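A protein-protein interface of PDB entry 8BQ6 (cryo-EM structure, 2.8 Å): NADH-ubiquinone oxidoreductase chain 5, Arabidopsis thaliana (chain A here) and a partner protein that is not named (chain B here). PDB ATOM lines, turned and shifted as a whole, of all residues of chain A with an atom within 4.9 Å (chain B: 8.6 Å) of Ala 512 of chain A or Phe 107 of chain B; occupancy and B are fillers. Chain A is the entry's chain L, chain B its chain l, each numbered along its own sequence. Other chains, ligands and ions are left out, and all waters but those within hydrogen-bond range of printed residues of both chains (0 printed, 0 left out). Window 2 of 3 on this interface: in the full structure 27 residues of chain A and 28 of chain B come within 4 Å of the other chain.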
ATOM      1  N   THR A 410     -23.857 -27.895  19.606  1.00  0.00           N
ATOM      2  CA  THR A 410     -23.748 -26.755  18.710  1.00  0.00           C
ATOM      3  C   THR A 410     -23.874 -25.418  19.429  1.00  0.00           C
ATOM      4  O   THR A 410     -23.385 -24.408  18.914  1.00  0.00           O
ATOM      5  CB  THR A 410     -24.807 -26.866  17.615  1.00  0.00           C
ATOM      6  OG1 THR A 410     -24.903 -28.233  17.198  1.00  0.00           O
ATOM      7  CG2 THR A 410     -24.425 -26.016  16.420  1.00  0.00           C
ATOM      8  N   TYR A 412     -22.559 -22.825  21.439  1.00  0.00           N
ATOM      9  CA  TYR A 412     -21.184 -22.497  21.813  1.00  0.00           C
ATOM     10  C   TYR A 412     -21.199 -21.456  22.930  1.00  0.00           C
ATOM     11  O   TYR A 412     -20.691 -20.341  22.817  1.00  0.00           O
ATOM     12  CB  TYR A 412     -20.409 -22.046  20.584  1.00  0.00           C
ATOM     13  CG  TYR A 412     -19.722 -23.206  19.911  1.00  0.00           C
ATOM     14  CD1 TYR A 412     -20.249 -23.777  18.764  1.00  0.00           C
ATOM     15  CD2 TYR A 412     -18.535 -23.712  20.406  1.00  0.00           C
ATOM     16  CE1 TYR A 412     -19.635 -24.842  18.156  1.00  0.00           C
ATOM     17  CE2 TYR A 412     -17.903 -24.768  19.794  1.00  0.00           C
ATOM     18  CZ  TYR A 412     -18.461 -25.333  18.671  1.00  0.00           C
ATOM     19  OH  TYR A 412     -17.840 -26.389  18.051  1.00  0.00           O
ATOM     20  N   ALA A 507     -29.391 -25.759  11.423  1.00  0.00           N
ATOM     21  CA  ALA A 507     -28.606 -26.111  10.243  1.00  0.00           C
ATOM     22  C   ALA A 507     -27.179 -26.487  10.625  1.00  0.00           C
ATOM     23  O   ALA A 507     -26.663 -27.525  10.194  1.00  0.00           O
ATOM     24  CB  ALA A 507     -28.618 -24.954   9.245  1.00  0.00           C
ATOM     25  N   GLU A 508     -26.545 -25.661  11.455  1.00  0.00           N
ATOM     26  CA  GLU A 508     -25.160 -25.956  11.914  1.00  0.00           C
ATOM     27  C   GLU A 508     -25.143 -27.257  12.729  1.00  0.00           C
ATOM     28  O   GLU A 508     -24.116 -27.951  12.694  1.00  0.00           O
ATOM     29  CB  GLU A 508     -24.612 -24.782  12.724  1.00  0.00           C
ATOM     30  CG  GLU A 508     -24.660 -23.459  11.989  1.00  0.00           C
ATOM     31  CD  GLU A 508     -25.794 -22.536  12.401  1.00  0.00           C
ATOM     32  OE1 GLU A 508     -26.945 -22.823  12.035  1.00  0.00           O
ATOM     33  OE2 GLU A 508     -25.521 -21.531  13.079  1.00  0.00           O
ATOM     34  N   GLU A 510     -26.824 -29.913  12.183  1.00  0.00           N
ATOM     35  CA  GLU A 510     -26.987 -31.070  11.316  1.00  0.00           C
ATOM     36  C   GLU A 510     -25.847 -31.226  10.313  1.00  0.00           C
ATOM     37  O   GLU A 510     -25.627 -32.338   9.822  1.00  0.00           O
ATOM     38  CB  GLU A 510     -28.342 -30.972  10.601  1.00  0.00           C
ATOM     39  CG  GLU A 510     -28.654 -32.033   9.543  1.00  0.00           C
ATOM     40  CD  GLU A 510     -28.855 -33.433  10.109  1.00  0.00           C
ATOM     41  OE1 GLU A 510     -29.819 -34.107   9.689  1.00  0.00           O
ATOM     42  OE2 GLU A 510     -28.041 -33.881  10.940  1.00  0.00           O
ATOM     43  N   PHE A 511     -25.085 -30.167  10.038  1.00  0.00           N
ATOM     44  CA  PHE A 511     -24.095 -30.219   8.969  1.00  0.00           C
ATOM     45  C   PHE A 511     -22.671 -29.982   9.461  1.00  0.00           C
ATOM     46  O   PHE A 511     -21.740 -30.656   9.010  1.00  0.00           O
ATOM     47  CB  PHE A 511     -24.468 -29.204   7.889  1.00  0.00           C
ATOM     48  CG  PHE A 511     -25.777 -29.502   7.221  1.00  0.00           C
ATOM     49  CD1 PHE A 511     -26.103 -30.796   6.855  1.00  0.00           C
ATOM     50  CD2 PHE A 511     -26.698 -28.494   6.993  1.00  0.00           C
ATOM     51  CE1 PHE A 511     -27.310 -31.074   6.250  1.00  0.00           C
ATOM     52  CE2 PHE A 511     -27.906 -28.766   6.394  1.00  0.00           C
ATOM     53  CZ  PHE A 511     -28.215 -30.057   6.022  1.00  0.00           C
ATOM     54  N   ALA A 512     -22.478 -29.043  10.387  1.00  0.00           N
ATOM     55  CA  ALA A 512     -21.142 -28.670  10.836  1.00  0.00           C
ATOM     56  C   ALA A 512     -20.627 -29.545  11.973  1.00  0.00           C
ATOM     57  O   ALA A 512     -19.538 -29.287  12.495  1.00  0.00           O
ATOM     58  CB  ALA A 512     -21.117 -27.201  11.263  1.00  0.00           C
ATOM     59  N   ALA A 513     -21.383 -30.563  12.372  1.00  0.00           N
ATOM     60  CA  ALA A 513     -20.975 -31.401  13.492  1.00  0.00           C
ATOM     61  C   ALA A 513     -20.130 -32.578  13.013  1.00  0.00           C
ATOM     62  O   ALA A 513     -20.459 -33.208  12.004  1.00  0.00           O
ATOM     63  CB  ALA A 513     -22.190 -31.930  14.239  1.00  0.00           C
ATOM     64  N   PRO A 514     -19.054 -32.888  13.735  1.00  0.00           N
ATOM     65  CA  PRO A 514     -18.294 -34.106  13.436  1.00  0.00           C
ATOM     66  C   PRO A 514     -19.178 -35.336  13.566  1.00  0.00           C
ATOM     67  O   PRO A 514     -20.095 -35.381  14.389  1.00  0.00           O
ATOM     68  CB  PRO A 514     -17.184 -34.102  14.493  1.00  0.00           C
ATOM     69  CG  PRO A 514     -17.062 -32.685  14.916  1.00  0.00           C
ATOM     70  CD  PRO A 514     -18.440 -32.101  14.816  1.00  0.00           C
ATOM     71  N   ALA B 102     -16.933 -21.032  23.739  1.00  0.00           N
ATOM     72  CA  ALA B 102     -17.317 -19.913  22.887  1.00  0.00           C
ATOM     73  C   ALA B 102     -16.152 -19.387  22.064  1.00  0.00           C
ATOM     74  O   ALA B 102     -16.371 -18.792  21.005  1.00  0.00           O
ATOM     75  CB  ALA B 102     -17.898 -18.782  23.735  1.00  0.00           C
ATOM     76  N   LYS B 104     -13.803 -21.232  20.635  1.00  0.00           N
ATOM     77  CA  LYS B 104     -13.398 -22.184  19.606  1.00  0.00           C
ATOM     78  C   LYS B 104     -14.541 -22.509  18.653  1.00  0.00           C
ATOM     79  O   LYS B 104     -14.688 -23.654  18.221  1.00  0.00           O
ATOM     80  CB  LYS B 104     -12.860 -23.470  20.228  1.00  0.00           C
ATOM     81  CG  LYS B 104     -13.853 -24.235  21.069  1.00  0.00           C
ATOM     82  CD  LYS B 104     -13.210 -25.484  21.630  1.00  0.00           C
ATOM     83  CE  LYS B 104     -12.145 -25.139  22.648  1.00  0.00           C
ATOM     84  NZ  LYS B 104     -11.507 -26.365  23.206  1.00  0.00           N
ATOM     85  N   VAL B 105     -15.321 -21.482  18.304  1.00  0.00           N
ATOM     86  CA  VAL B 105     -16.482 -21.679  17.386  1.00  0.00           C
ATOM     87  C   VAL B 105     -15.935 -21.914  15.974  1.00  0.00           C
ATOM     88  O   VAL B 105     -15.086 -21.121  15.533  1.00  0.00           O
ATOM     89  CB  VAL B 105     -17.476 -20.498  17.479  1.00  0.00           C
ATOM     90  CG1 VAL B 105     -16.807 -19.133  17.481  1.00  0.00           C
ATOM     91  CG2 VAL B 105     -18.603 -20.566  16.467  1.00  0.00           C
ATOM     92  N   PRO B 106     -16.350 -22.980  15.257  1.00  0.00           N
ATOM     93  CA  PRO B 106     -15.795 -23.301  13.943  1.00  0.00           C
ATOM     94  C   PRO B 106     -16.535 -22.652  12.762  1.00  0.00           C
ATOM     95  O   PRO B 106     -16.300 -23.087  11.662  1.00  0.00           O
ATOM     96  CB  PRO B 106     -15.958 -24.826  13.911  1.00  0.00           C
ATOM     97  CG  PRO B 106     -17.261 -25.067  14.633  1.00  0.00           C
ATOM     98  CD  PRO B 106     -17.352 -23.961  15.663  1.00  0.00           C
ATOM     99  N   PHE B 107     -17.369 -21.639  13.006  1.00  0.00           N
ATOM    100  CA  PHE B 107     -18.043 -20.904  11.899  1.00  0.00           C
ATOM    101  C   PHE B 107     -18.228 -19.437  12.302  1.00  0.00           C
ATOM    102  O   PHE B 107     -18.138 -19.123  13.502  1.00  0.00           O
ATOM    103  CB  PHE B 107     -19.380 -21.540  11.500  1.00  0.00           C
ATOM    104  CG  PHE B 107     -20.156 -22.205  12.606  1.00  0.00           C
ATOM    105  CD1 PHE B 107     -20.864 -21.453  13.530  1.00  0.00           C
ATOM    106  CD2 PHE B 107     -20.199 -23.585  12.710  1.00  0.00           C
ATOM    107  CE1 PHE B 107     -21.581 -22.067  14.545  1.00  0.00           C
ATOM    108  CE2 PHE B 107     -20.913 -24.197  13.727  1.00  0.00           C
ATOM    109  CZ  PHE B 107     -21.602 -23.438  14.643  1.00  0.00           C
ATOM    110  N   THR B 108     -18.459 -18.564  11.318  1.00  0.00           N
ATOM    111  CA  THR B 108     -18.701 -17.125  11.615  1.00  0.00           C
ATOM    112  C   THR B 108     -20.183 -16.905  11.933  1.00  0.00           C
ATOM    113  O   THR B 108     -21.029 -17.610  11.349  1.00  0.00           O
ATOM    114  CB  THR B 108     -18.235 -16.228  10.463  1.00  0.00           C
ATOM    115  OG1 THR B 108     -18.921 -16.616   9.272  1.00  0.00           O
ATOM    116  CG2 THR B 108     -16.741 -16.292  10.241  1.00  0.00           C
ATOM    117  N   PRO B 109     -20.529 -15.970  12.843  1.00  0.00           N
ATOM    118  CA  PRO B 109     -21.927 -15.666  13.157  1.00  0.00           C
ATOM    119  C   PRO B 109     -22.804 -15.457  11.912  1.00  0.00           C
ATOM    120  O   PRO B 109     -22.396 -14.706  11.051  1.00  0.00           O
ATOM    121  CB  PRO B 109     -21.779 -14.337  13.908  1.00  0.00           C
ATOM    122  CG  PRO B 109     -20.483 -14.486  14.651  1.00  0.00           C
ATOM    123  CD  PRO B 109     -19.588 -15.201  13.664  1.00  0.00           C
ATOM    124  N   ARG B 110     -23.981 -16.096  11.856  1.00  0.00           N
ATOM    125  CA  ARG B 110     -24.889 -15.911  10.736  1.00  0.00           C
ATOM    126  C   ARG B 110     -25.083 -14.432  10.449  1.00  0.00           C
ATOM    127  O   ARG B 110     -25.188 -13.602  11.356  1.00  0.00           O
ATOM    128  CB  ARG B 110     -26.244 -16.548  11.021  1.00  0.00           C
ATOM    129  CG  ARG B 110     -26.294 -18.043  10.846  1.00  0.00           C
ATOM    130  CD  ARG B 110     -27.599 -18.551  11.403  1.00  0.00           C
ATOM    131  NE  ARG B 110     -27.830 -19.960  11.125  1.00  0.00           N
ATOM    132  CZ  ARG B 110     -28.956 -20.435  10.614  1.00  0.00           C
ATOM    133  NH1 ARG B 110     -29.939 -19.630  10.245  1.00  0.00           N
ATOM    134  NH2 ARG B 110     -29.101 -21.748  10.468  1.00  0.00           N
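The guanidinium group (NH2) of Arg 110 of chain B is in salt-bridge range of the side-chain carboxylate (OE1) of Glu 508 of chain A (2.9 Å).
Among the printed residues, merely in contact across the chains: Tyr 412 of chain A with Ala 102 of chain B, Tyr 412 of chain A with Lys 104 of chain B, Tyr 412 of chain A with Pro 106 of chain B, Ala 507 of chain A with Arg 110 of chain B, Glu 508 of chain A with Phe 107 of chain B and Ala 512 of chain A with Phe 107 of chain B.
Printed residues of chain B within 4 Å of Glu 508 of chain A: Phe 107 and Arg 110. Of chain B, only Phe 107 comes within 4 Å of Ala 512 of chain A. No residue of chain B comes within 4 Å of Ala 513 of chain A. Val 105 of chain B touches none of the printed residues of chain A. Printed residues of chain A within 4 Å of Pro 106 of chain B: Tyr 412. Phe 107 of chain B touches just these residues of chain A: Glu 508 and Ala 512. Pro 109 of chain B touches none of the printed residues of chain A. The nearest residue of chain B that does not touch Ala 512 of chain A is Pro 106 of chain B (5.3 Å).
Of the 9 printed residues of chain A, 4 touch a printed residue of chain B. Hydrophobic or aromatic side chains of chain A within 4 Å of the printed part of chain B: Tyr 412, Ala 507 and Ala 512. Among the printed residues, 7 pairs touch across the chains.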
